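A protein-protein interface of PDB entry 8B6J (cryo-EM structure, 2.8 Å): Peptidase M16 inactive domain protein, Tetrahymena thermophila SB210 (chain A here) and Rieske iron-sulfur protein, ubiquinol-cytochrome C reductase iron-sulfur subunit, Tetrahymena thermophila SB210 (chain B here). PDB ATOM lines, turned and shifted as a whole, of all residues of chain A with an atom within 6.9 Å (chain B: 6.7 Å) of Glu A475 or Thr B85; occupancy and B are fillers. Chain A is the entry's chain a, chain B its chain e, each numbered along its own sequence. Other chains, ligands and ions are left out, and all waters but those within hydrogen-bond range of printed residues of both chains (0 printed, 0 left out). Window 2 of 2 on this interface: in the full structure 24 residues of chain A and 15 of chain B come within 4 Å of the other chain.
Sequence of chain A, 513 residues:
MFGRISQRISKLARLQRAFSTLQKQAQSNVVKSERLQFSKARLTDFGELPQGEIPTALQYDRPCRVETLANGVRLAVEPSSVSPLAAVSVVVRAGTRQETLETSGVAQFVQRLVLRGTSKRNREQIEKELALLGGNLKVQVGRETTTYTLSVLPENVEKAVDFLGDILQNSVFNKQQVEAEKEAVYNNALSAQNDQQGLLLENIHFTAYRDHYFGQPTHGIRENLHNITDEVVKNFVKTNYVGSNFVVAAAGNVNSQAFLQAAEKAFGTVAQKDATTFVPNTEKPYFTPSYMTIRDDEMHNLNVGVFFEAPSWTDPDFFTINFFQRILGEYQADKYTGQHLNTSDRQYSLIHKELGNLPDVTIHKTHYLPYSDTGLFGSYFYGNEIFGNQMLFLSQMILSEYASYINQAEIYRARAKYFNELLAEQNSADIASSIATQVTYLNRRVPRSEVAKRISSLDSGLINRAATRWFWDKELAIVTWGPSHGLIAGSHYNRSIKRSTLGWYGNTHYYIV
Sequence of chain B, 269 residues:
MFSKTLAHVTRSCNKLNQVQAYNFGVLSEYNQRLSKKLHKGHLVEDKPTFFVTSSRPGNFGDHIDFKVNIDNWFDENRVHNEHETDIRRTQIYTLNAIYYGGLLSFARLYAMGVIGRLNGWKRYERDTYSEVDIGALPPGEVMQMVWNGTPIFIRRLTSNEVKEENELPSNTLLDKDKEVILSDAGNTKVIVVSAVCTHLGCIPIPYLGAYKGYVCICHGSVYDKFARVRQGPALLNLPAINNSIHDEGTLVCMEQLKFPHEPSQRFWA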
ATOM      1  N   PHE A 287       1.425  20.164  19.533  1.00  0.00           N
ATOM      2  CA  PHE A 287       0.634  21.213  18.905  1.00  0.00           C
ATOM      3  C   PHE A 287      -0.192  20.641  17.761  1.00  0.00           C
ATOM      4  O   PHE A 287       0.318  19.883  16.930  1.00  0.00           O
ATOM      5  CB  PHE A 287       1.564  22.316  18.400  1.00  0.00           C
ATOM      6  CG  PHE A 287       0.854  23.464  17.745  1.00  0.00           C
ATOM      7  CD1 PHE A 287       0.082  24.335  18.489  1.00  0.00           C
ATOM      8  CD2 PHE A 287       0.983  23.685  16.386  1.00  0.00           C
ATOM      9  CE1 PHE A 287      -0.563  25.395  17.886  1.00  0.00           C
ATOM     10  CE2 PHE A 287       0.341  24.743  15.780  1.00  0.00           C
ATOM     11  CZ  PHE A 287      -0.432  25.599  16.531  1.00  0.00           C
ATOM     12  N   THR A 288      -1.470  21.010  17.716  1.00  0.00           N
ATOM     13  CA  THR A 288      -2.401  20.520  16.698  1.00  0.00           C
ATOM     14  C   THR A 288      -2.923  21.692  15.881  1.00  0.00           C
ATOM     15  O   THR A 288      -3.880  22.368  16.301  1.00  0.00           O
ATOM     16  CB  THR A 288      -3.561  19.764  17.345  1.00  0.00           C
ATOM     17  OG1 THR A 288      -3.052  18.680  18.131  1.00  0.00           O
ATOM     18  CG2 THR A 288      -4.500  19.214  16.285  1.00  0.00           C
ATOM     19  N   PRO A 289      -2.340  21.980  14.716  1.00  0.00           N
ATOM     20  CA  PRO A 289      -2.836  23.101  13.907  1.00  0.00           C
ATOM     21  C   PRO A 289      -4.300  22.916  13.541  1.00  0.00           C
ATOM     22  O   PRO A 289      -4.738  21.816  13.201  1.00  0.00           O
ATOM     23  CB  PRO A 289      -1.935  23.067  12.668  1.00  0.00           C
ATOM     24  CG  PRO A 289      -0.710  22.350  13.106  1.00  0.00           C
ATOM     25  CD  PRO A 289      -1.159  21.344  14.112  1.00  0.00           C
ATOM     26  N   SER A 290      -5.055  24.009  13.603  1.00  0.00           N
ATOM     27  CA  SER A 290      -6.487  23.955  13.347  1.00  0.00           C
ATOM     28  C   SER A 290      -7.004  25.370  13.126  1.00  0.00           C
ATOM     29  O   SER A 290      -6.298  26.356  13.353  1.00  0.00           O
ATOM     30  CB  SER A 290      -7.235  23.281  14.500  1.00  0.00           C
ATOM     31  OG  SER A 290      -6.866  21.920  14.625  1.00  0.00           O
ATOM     32  N   PHE A 307      -2.059  31.981  16.452  1.00  0.00           N
ATOM     33  CA  PHE A 307      -0.951  31.611  17.318  1.00  0.00           C
ATOM     34  C   PHE A 307      -0.071  30.568  16.647  1.00  0.00           C
ATOM     35  O   PHE A 307      -0.533  29.768  15.830  1.00  0.00           O
ATOM     36  CB  PHE A 307      -1.458  31.068  18.664  1.00  0.00           C
ATOM     37  CG  PHE A 307      -1.894  32.141  19.620  1.00  0.00           C
ATOM     38  CD1 PHE A 307      -2.998  32.928  19.346  1.00  0.00           C
ATOM     39  CD2 PHE A 307      -1.198  32.361  20.796  1.00  0.00           C
ATOM     40  CE1 PHE A 307      -3.395  33.916  20.221  1.00  0.00           C
ATOM     41  CE2 PHE A 307      -1.594  33.345  21.674  1.00  0.00           C
ATOM     42  CZ  PHE A 307      -2.693  34.123  21.387  1.00  0.00           C
ATOM     43  N   PHE A 308       1.209  30.595  17.001  1.00  0.00           N
ATOM     44  CA  PHE A 308       2.186  29.596  16.609  1.00  0.00           C
ATOM     45  C   PHE A 308       2.636  28.830  17.844  1.00  0.00           C
ATOM     46  O   PHE A 308       2.575  29.338  18.970  1.00  0.00           O
ATOM     47  CB  PHE A 308       3.418  30.231  15.953  1.00  0.00           C
ATOM     48  CG  PHE A 308       3.104  31.220  14.869  1.00  0.00           C
ATOM     49  CD1 PHE A 308       2.630  32.484  15.180  1.00  0.00           C
ATOM     50  CD2 PHE A 308       3.321  30.902  13.542  1.00  0.00           C
ATOM     51  CE1 PHE A 308       2.353  33.398  14.186  1.00  0.00           C
ATOM     52  CE2 PHE A 308       3.049  31.813  12.545  1.00  0.00           C
ATOM     53  CZ  PHE A 308       2.564  33.062  12.867  1.00  0.00           C
ATOM     54  N   GLU A 309       3.093  27.601  17.623  1.00  0.00           N
ATOM     55  CA  GLU A 309       3.776  26.870  18.678  1.00  0.00           C
ATOM     56  C   GLU A 309       5.012  27.648  19.106  1.00  0.00           C
ATOM     57  O   GLU A 309       5.791  28.108  18.266  1.00  0.00           O
ATOM     58  CB  GLU A 309       4.164  25.476  18.188  1.00  0.00           C
ATOM     59  CG  GLU A 309       4.814  24.602  19.244  1.00  0.00           C
ATOM     60  CD  GLU A 309       5.230  23.253  18.700  1.00  0.00           C
ATOM     61  OE1 GLU A 309       5.325  23.114  17.463  1.00  0.00           O
ATOM     62  OE2 GLU A 309       5.458  22.329  19.509  1.00  0.00           O
ATOM     63  N   TRP A 470      11.113  29.697  14.096  1.00  0.00           N
ATOM     64  CA  TRP A 470       9.845  29.562  14.801  1.00  0.00           C
ATOM     65  C   TRP A 470       8.626  30.058  14.038  1.00  0.00           C
ATOM     66  O   TRP A 470       7.519  29.595  14.328  1.00  0.00           O
ATOM     67  CB  TRP A 470       9.908  30.297  16.147  1.00  0.00           C
ATOM     68  CG  TRP A 470      10.719  29.569  17.168  1.00  0.00           C
ATOM     69  CD1 TRP A 470      11.984  29.866  17.575  1.00  0.00           C
ATOM     70  CD2 TRP A 470      10.322  28.407  17.904  1.00  0.00           C
ATOM     71  NE1 TRP A 470      12.399  28.966  18.524  1.00  0.00           N
ATOM     72  CE2 TRP A 470      11.397  28.058  18.743  1.00  0.00           C
ATOM     73  CE3 TRP A 470       9.162  27.630  17.936  1.00  0.00           C
ATOM     74  CZ2 TRP A 470      11.345  26.968  19.605  1.00  0.00           C
ATOM     75  CZ3 TRP A 470       9.113  26.548  18.792  1.00  0.00           C
ATOM     76  CH2 TRP A 470      10.198  26.227  19.615  1.00  0.00           C
ATOM     77  N   PHE A 471       8.782  30.973  13.082  1.00  0.00           N
ATOM     78  CA  PHE A 471       7.628  31.594  12.441  1.00  0.00           C
ATOM     79  C   PHE A 471       7.537  31.371  10.939  1.00  0.00           C
ATOM     80  O   PHE A 471       6.426  31.345  10.409  1.00  0.00           O
ATOM     81  CB  PHE A 471       7.621  33.107  12.708  1.00  0.00           C
ATOM     82  CG  PHE A 471       7.530  33.462  14.164  1.00  0.00           C
ATOM     83  CD1 PHE A 471       6.395  33.162  14.893  1.00  0.00           C
ATOM     84  CD2 PHE A 471       8.578  34.100  14.802  1.00  0.00           C
ATOM     85  CE1 PHE A 471       6.311  33.486  16.230  1.00  0.00           C
ATOM     86  CE2 PHE A 471       8.497  34.425  16.138  1.00  0.00           C
ATOM     87  CZ  PHE A 471       7.362  34.119  16.852  1.00  0.00           C
ATOM     88  N   TRP A 472       8.654  31.207  10.238  1.00  0.00           N
ATOM     89  CA  TRP A 472       8.602  31.129   8.784  1.00  0.00           C
ATOM     90  C   TRP A 472       8.016  29.799   8.330  1.00  0.00           C
ATOM     91  O   TRP A 472       8.483  28.731   8.734  1.00  0.00           O
ATOM     92  CB  TRP A 472       9.995  31.310   8.187  1.00  0.00           C
ATOM     93  CG  TRP A 472      10.012  31.185   6.698  1.00  0.00           C
ATOM     94  CD1 TRP A 472      10.295  30.068   5.974  1.00  0.00           C
ATOM     95  CD2 TRP A 472       9.724  32.217   5.747  1.00  0.00           C
ATOM     96  NE1 TRP A 472      10.205  30.338   4.630  1.00  0.00           N
ATOM     97  CE2 TRP A 472       9.855  31.651   4.465  1.00  0.00           C
ATOM     98  CE3 TRP A 472       9.368  33.564   5.856  1.00  0.00           C
ATOM     99  CZ2 TRP A 472       9.646  32.385   3.302  1.00  0.00           C
ATOM    100  CZ3 TRP A 472       9.162  34.289   4.701  1.00  0.00           C
ATOM    101  CH2 TRP A 472       9.300  33.699   3.441  1.00  0.00           C
ATOM    102  N   ASP A 473       6.995  29.871   7.477  1.00  0.00           N
ATOM    103  CA  ASP A 473       6.431  28.690   6.825  1.00  0.00           C
ATOM    104  C   ASP A 473       6.050  27.623   7.848  1.00  0.00           C
ATOM    105  O   ASP A 473       6.278  26.429   7.647  1.00  0.00           O
ATOM    106  CB  ASP A 473       7.408  28.130   5.793  1.00  0.00           C
ATOM    107  CG  ASP A 473       6.748  27.174   4.825  1.00  0.00           C
ATOM    108  OD1 ASP A 473       5.524  26.956   4.943  1.00  0.00           O
ATOM    109  OD2 ASP A 473       7.454  26.643   3.942  1.00  0.00           O
ATOM    110  N   LYS A 474       5.459  28.060   8.954  1.00  0.00           N
ATOM    111  CA  LYS A 474       5.094  27.185  10.057  1.00  0.00           C
ATOM    112  C   LYS A 474       3.579  27.061  10.158  1.00  0.00           C
ATOM    113  O   LYS A 474       2.827  27.858   9.593  1.00  0.00           O
ATOM    114  CB  LYS A 474       5.669  27.710  11.378  1.00  0.00           C
ATOM    115  CG  LYS A 474       6.425  26.667  12.192  1.00  0.00           C
ATOM    116  CD  LYS A 474       7.688  26.176  11.487  1.00  0.00           C
ATOM    117  CE  LYS A 474       8.770  27.240  11.447  1.00  0.00           C
ATOM    118  NZ  LYS A 474       9.958  26.791  10.673  1.00  0.00           N
ATOM    119  N   GLU A 475       3.140  26.040  10.889  1.00  0.00           N
ATOM    120  CA  GLU A 475       1.719  25.796  11.066  1.00  0.00           C
ATOM    121  C   GLU A 475       1.114  26.833  12.011  1.00  0.00           C
ATOM    122  O   GLU A 475       1.819  27.582  12.694  1.00  0.00           O
ATOM    123  CB  GLU A 475       1.482  24.386  11.602  1.00  0.00           C
ATOM    124  CG  GLU A 475       2.030  23.280  10.715  1.00  0.00           C
ATOM    125  CD  GLU A 475       1.299  23.169   9.392  1.00  0.00           C
ATOM    126  OE1 GLU A 475       0.292  23.882   9.205  1.00  0.00           O
ATOM    127  OE2 GLU A 475       1.730  22.367   8.540  1.00  0.00           O
ATOM    128  N   LEU A 476      -0.217  26.865  12.052  1.00  0.00           N
ATOM    129  CA  LEU A 476      -0.957  27.883  12.782  1.00  0.00           C
ATOM    130  C   LEU A 476      -2.082  27.258  13.592  1.00  0.00           C
ATOM    131  O   LEU A 476      -2.586  26.179  13.273  1.00  0.00           O
ATOM    132  CB  LEU A 476      -1.557  28.930  11.834  1.00  0.00           C
ATOM    133  CG  LEU A 476      -0.607  29.949  11.215  1.00  0.00           C
ATOM    134  CD1 LEU A 476      -1.330  30.751  10.152  1.00  0.00           C
ATOM    135  CD2 LEU A 476      -0.048  30.863  12.283  1.00  0.00           C
ATOM    136  N   ALA A 477      -2.469  27.963  14.651  1.00  0.00           N
ATOM    137  CA  ALA A 477      -3.704  27.710  15.381  1.00  0.00           C
ATOM    138  C   ALA A 477      -4.538  28.980  15.316  1.00  0.00           C
ATOM    139  O   ALA A 477      -4.128  30.019  15.843  1.00  0.00           O
ATOM    140  CB  ALA A 477      -3.428  27.314  16.831  1.00  0.00           C
ATOM    141  N   TYR A 493      -8.867  25.330   6.580  1.00  0.00           N
ATOM    142  CA  TYR A 493      -7.414  25.444   6.492  1.00  0.00           C
ATOM    143  C   TYR A 493      -7.000  25.152   5.056  1.00  0.00           C
ATOM    144  O   TYR A 493      -6.908  23.993   4.647  1.00  0.00           O
ATOM    145  CB  TYR A 493      -6.752  24.481   7.469  1.00  0.00           C
ATOM    146  CG  TYR A 493      -5.386  24.913   7.942  1.00  0.00           C
ATOM    147  CD1 TYR A 493      -4.288  24.861   7.099  1.00  0.00           C
ATOM    148  CD2 TYR A 493      -5.193  25.363   9.239  1.00  0.00           C
ATOM    149  CE1 TYR A 493      -3.039  25.252   7.530  1.00  0.00           C
ATOM    150  CE2 TYR A 493      -3.947  25.755   9.680  1.00  0.00           C
ATOM    151  CZ  TYR A 493      -2.874  25.698   8.822  1.00  0.00           C
ATOM    152  OH  TYR A 493      -1.631  26.088   9.258  1.00  0.00           O
ATOM    153  N   LYS A 498      -2.291  28.518   4.468  1.00  0.00           N
ATOM    154  CA  LYS A 498      -1.003  27.836   4.410  1.00  0.00           C
ATOM    155  C   LYS A 498       0.127  28.811   4.113  1.00  0.00           C
ATOM    156  O   LYS A 498       1.194  28.744   4.734  1.00  0.00           O
ATOM    157  CB  LYS A 498      -1.052  26.736   3.351  1.00  0.00           C
ATOM    158  CG  LYS A 498       0.161  25.829   3.322  1.00  0.00           C
ATOM    159  CD  LYS A 498       0.073  24.843   2.169  1.00  0.00           C
ATOM    160  CE  LYS A 498       1.087  23.721   2.308  1.00  0.00           C
ATOM    161  NZ  LYS A 498       0.800  22.847   3.481  1.00  0.00           N
ATOM    162  N   THR A 501       1.780  32.276   6.713  1.00  0.00           N
ATOM    163  CA  THR A 501       2.981  32.275   7.538  1.00  0.00           C
ATOM    164  C   THR A 501       4.245  32.542   6.733  1.00  0.00           C
ATOM    165  O   THR A 501       5.315  32.694   7.329  1.00  0.00           O
ATOM    166  CB  THR A 501       3.114  30.945   8.274  1.00  0.00           C
ATOM    167  OG1 THR A 501       3.099  29.869   7.329  1.00  0.00           O
ATOM    168  CG2 THR A 501       1.974  30.770   9.257  1.00  0.00           C
ATOM    169  N   ASN B  81       0.526  12.405  13.274  1.00  0.00           N
ATOM    170  CA  ASN B  81       1.885  12.928  13.236  1.00  0.00           C
ATOM    171  C   ASN B  81       1.895  14.398  13.627  1.00  0.00           C
ATOM    172  O   ASN B  81       2.485  15.244  12.952  1.00  0.00           O
ATOM    173  CB  ASN B  81       2.501  12.737  11.853  1.00  0.00           C
ATOM    174  CG  ASN B  81       1.821  13.577  10.792  1.00  0.00           C
ATOM    175  OD1 ASN B  81       0.681  14.003  10.961  1.00  0.00           O
ATOM    176  ND2 ASN B  81       2.521  13.820   9.692  1.00  0.00           N
ATOM    177  N   GLU B  82       1.216  14.728  14.728  1.00  0.00           N
ATOM    178  CA  GLU B  82       1.272  16.094  15.238  1.00  0.00           C
ATOM    179  C   GLU B  82       2.719  16.541  15.380  1.00  0.00           C
ATOM    180  O   GLU B  82       3.085  17.653  14.979  1.00  0.00           O
ATOM    181  CB  GLU B  82       0.538  16.189  16.576  1.00  0.00           C
ATOM    182  CG  GLU B  82      -0.963  16.386  16.443  1.00  0.00           C
ATOM    183  CD  GLU B  82      -1.638  15.266  15.681  1.00  0.00           C
ATOM    184  OE1 GLU B  82      -0.969  14.249  15.402  1.00  0.00           O
ATOM    185  OE2 GLU B  82      -2.837  15.400  15.358  1.00  0.00           O
ATOM    186  N   HIS B  83       3.557  15.683  15.952  1.00  0.00           N
ATOM    187  CA  HIS B  83       4.994  15.824  15.788  1.00  0.00           C
ATOM    188  C   HIS B  83       5.370  15.494  14.350  1.00  0.00           C
ATOM    189  O   HIS B  83       4.769  14.623  13.716  1.00  0.00           O
ATOM    190  CB  HIS B  83       5.736  14.889  16.738  1.00  0.00           C
ATOM    191  CG  HIS B  83       5.702  13.455  16.310  1.00  0.00           C
ATOM    192  ND1 HIS B  83       4.646  12.618  16.594  1.00  0.00           N
ATOM    193  CD2 HIS B  83       6.590  12.714  15.606  1.00  0.00           C
ATOM    194  CE1 HIS B  83       4.886  11.421  16.089  1.00  0.00           C
ATOM    195  NE2 HIS B  83       6.061  11.452  15.485  1.00  0.00           N
ATOM    196  N   GLU B  84       6.375  16.196  13.831  1.00  0.00           N
ATOM    197  CA  GLU B  84       6.865  15.958  12.477  1.00  0.00           C
ATOM    198  C   GLU B  84       5.886  16.467  11.421  1.00  0.00           C
ATOM    199  O   GLU B  84       5.824  15.934  10.312  1.00  0.00           O
ATOM    200  CB  GLU B  84       7.144  14.466  12.261  1.00  0.00           C
ATOM    201  CG  GLU B  84       8.092  14.148  11.126  1.00  0.00           C
ATOM    202  CD  GLU B  84       7.975  12.708  10.669  1.00  0.00           C
ATOM    203  OE1 GLU B  84       6.846  12.173  10.668  1.00  0.00           O
ATOM    204  OE2 GLU B  84       9.010  12.105  10.315  1.00  0.00           O
ATOM    205  N   THR B  85       5.107  17.498  11.756  1.00  0.00           N
ATOM    206  CA  THR B  85       4.155  18.051  10.796  1.00  0.00           C
ATOM    207  C   THR B  85       4.872  18.705   9.622  1.00  0.00           C
ATOM    208  O   THR B  85       4.409  18.625   8.476  1.00  0.00           O
ATOM    209  CB  THR B  85       3.245  19.063  11.491  1.00  0.00           C
ATOM    210  OG1 THR B  85       2.634  18.456  12.635  1.00  0.00           O
ATOM    211  CG2 THR B  85       2.162  19.551  10.544  1.00  0.00           C
ATOM    212  N   ASP B  86       6.001  19.361   9.890  1.00  0.00           N
ATOM    213  CA  ASP B  86       6.718  20.062   8.832  1.00  0.00           C
ATOM    214  C   ASP B  86       7.167  19.111   7.731  1.00  0.00           C
ATOM    215  O   ASP B  86       7.251  19.512   6.566  1.00  0.00           O
ATOM    216  CB  ASP B  86       7.917  20.799   9.421  1.00  0.00           C
ATOM    217  CG  ASP B  86       7.508  21.901  10.380  1.00  0.00           C
ATOM    218  OD1 ASP B  86       6.446  22.519  10.160  1.00  0.00           O
ATOM    219  OD2 ASP B  86       8.247  22.147  11.356  1.00  0.00           O
ATOM    220  N   ILE B  87       7.456  17.854   8.068  1.00  0.00           N
ATOM    221  CA  ILE B  87       7.832  16.895   7.036  1.00  0.00           C
ATOM    222  C   ILE B  87       6.661  16.639   6.095  1.00  0.00           C
ATOM    223  O   ILE B  87       6.834  16.571   4.873  1.00  0.00           O
ATOM    224  CB  ILE B  87       8.352  15.595   7.675  1.00  0.00           C
ATOM    225  CG1 ILE B  87       9.614  15.901   8.488  1.00  0.00           C
ATOM    226  CG2 ILE B  87       8.618  14.542   6.602  1.00  0.00           C
ATOM    227  CD1 ILE B  87      10.407  14.687   8.911  1.00  0.00           C
ATOM    228  N   ARG B  88       5.452  16.491   6.642  1.00  0.00           N
ATOM    229  CA  ARG B  88       4.285  16.316   5.785  1.00  0.00           C
ATOM    230  C   ARG B  88       4.029  17.564   4.949  1.00  0.00           C
ATOM    231  O   ARG B  88       3.626  17.471   3.782  1.00  0.00           O
ATOM    232  CB  ARG B  88       3.059  15.966   6.630  1.00  0.00           C
ATOM    233  CG  ARG B  88       1.753  15.888   5.847  1.00  0.00           C
ATOM    234  CD  ARG B  88       1.837  14.934   4.664  1.00  0.00           C
ATOM    235  NE  ARG B  88       2.032  13.549   5.076  1.00  0.00           N
ATOM    236  CZ  ARG B  88       1.056  12.667   5.252  1.00  0.00           C
ATOM    237  NH1 ARG B  88      -0.214  12.993   5.076  1.00  0.00           N
ATOM    238  NH2 ARG B  88       1.363  11.425   5.612  1.00  0.00           N
ATOM    239  N   ARG B  89       4.256  18.744   5.529  1.00  0.00           N
ATOM    240  CA  ARG B  89       4.118  19.975   4.755  1.00  0.00           C
ATOM    241  C   ARG B  89       5.101  20.001   3.590  1.00  0.00           C
ATOM    242  O   ARG B  89       4.746  20.391   2.471  1.00  0.00           O
ATOM    243  CB  ARG B  89       4.320  21.186   5.665  1.00  0.00           C
ATOM    244  CG  ARG B  89       4.020  22.521   5.004  1.00  0.00           C
ATOM    245  CD  ARG B  89       3.670  23.578   6.038  1.00  0.00           C
ATOM    246  NE  ARG B  89       3.327  24.857   5.428  1.00  0.00           N
ATOM    247  CZ  ARG B  89       2.717  25.851   6.060  1.00  0.00           C
ATOM    248  NH1 ARG B  89       2.347  25.743   7.325  1.00  0.00           N
ATOM    249  NH2 ARG B  89       2.468  26.980   5.405  1.00  0.00           N
ATOM    250  N   THR B  90       6.345  19.586   3.835  1.00  0.00           N
ATOM    251  CA  THR B  90       7.333  19.517   2.763  1.00  0.00           C
ATOM    252  C   THR B  90       6.925  18.502   1.703  1.00  0.00           C
ATOM    253  O   THR B  90       7.144  18.719   0.508  1.00  0.00           O
ATOM    254  CB  THR B  90       8.707  19.166   3.332  1.00  0.00           C
ATOM    255  OG1 THR B  90       9.073  20.125   4.332  1.00  0.00           O
ATOM    256  CG2 THR B  90       9.754  19.163   2.232  1.00  0.00           C
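The backbone carbonyl oxygen (O) of Thr A288 sits at hydrogen-bond distance from the side-chain hydroxyl (OG) of Ser A290, at 3.5 Å. NZ of Lys A474 lies close to O of Trp A472, at 3.1 Å. O of Lys A474 is in hydrogen-bond range of OG1 of Thr A501 (3.0 Å). OE1 of Glu A475 lies within hydrogen-bond range of OH of Tyr A493 (2.9 Å). The side-chain hydroxyl of Thr A501 is in hydrogen-bond range of the backbone carbonyl oxygen of Lys A498, at 3.4 Å. The side-chain hydroxyl (OG1) of Thr B85 sits at hydrogen-bond distance from the backbone carbonyl oxygen (O) of Glu B82, 2.5 Å away.
OD1 of Asp A473 is in salt-bridge range of NE of Arg B89 (3.1 Å). The backbone carbonyl oxygen (O) of Lys A474 is in hydrogen-bond range of the guanidinium group (NH1) of Arg B89, 3.1 Å away. NH1 of Arg B89 lies within salt-bridge range of OE1 of Glu A475 (3.3 Å). O of Lys A498 lies close to NH2 of Arg B89, 2.3 Å away.
Printed residues of chain B within 4 Å of Thr A288: Glu B82 (3.5 Å). Glu A475 touches two residues of chain B. Printed residues of chain B within 4 Å of Lys A498: Arg B89. Of the printed residues of chain A, Thr B85 touches Glu A475. The nearest residue of chain B that does not touch Glu A475 is Asp B86 (4.5 Å). The nearest printed residue of chain A that does not touch Glu B82 is Pro A289 (5.5 Å).
Phe A287 touches Glu B82. OG1 of Thr A288 touches CG of Glu B82, 3.5 Å away. Glu A475 touches Thr B85. OG1 of Thr A501 touches NH2 of Arg B89, 3.5 Å away.
Of the 18 printed residues of chain A, 7 touch a printed residue of chain B. Of the 10 printed residues of chain B, 3 touch a printed residue of chain A. Among the printed residues, 8 pairs touch across the chains.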
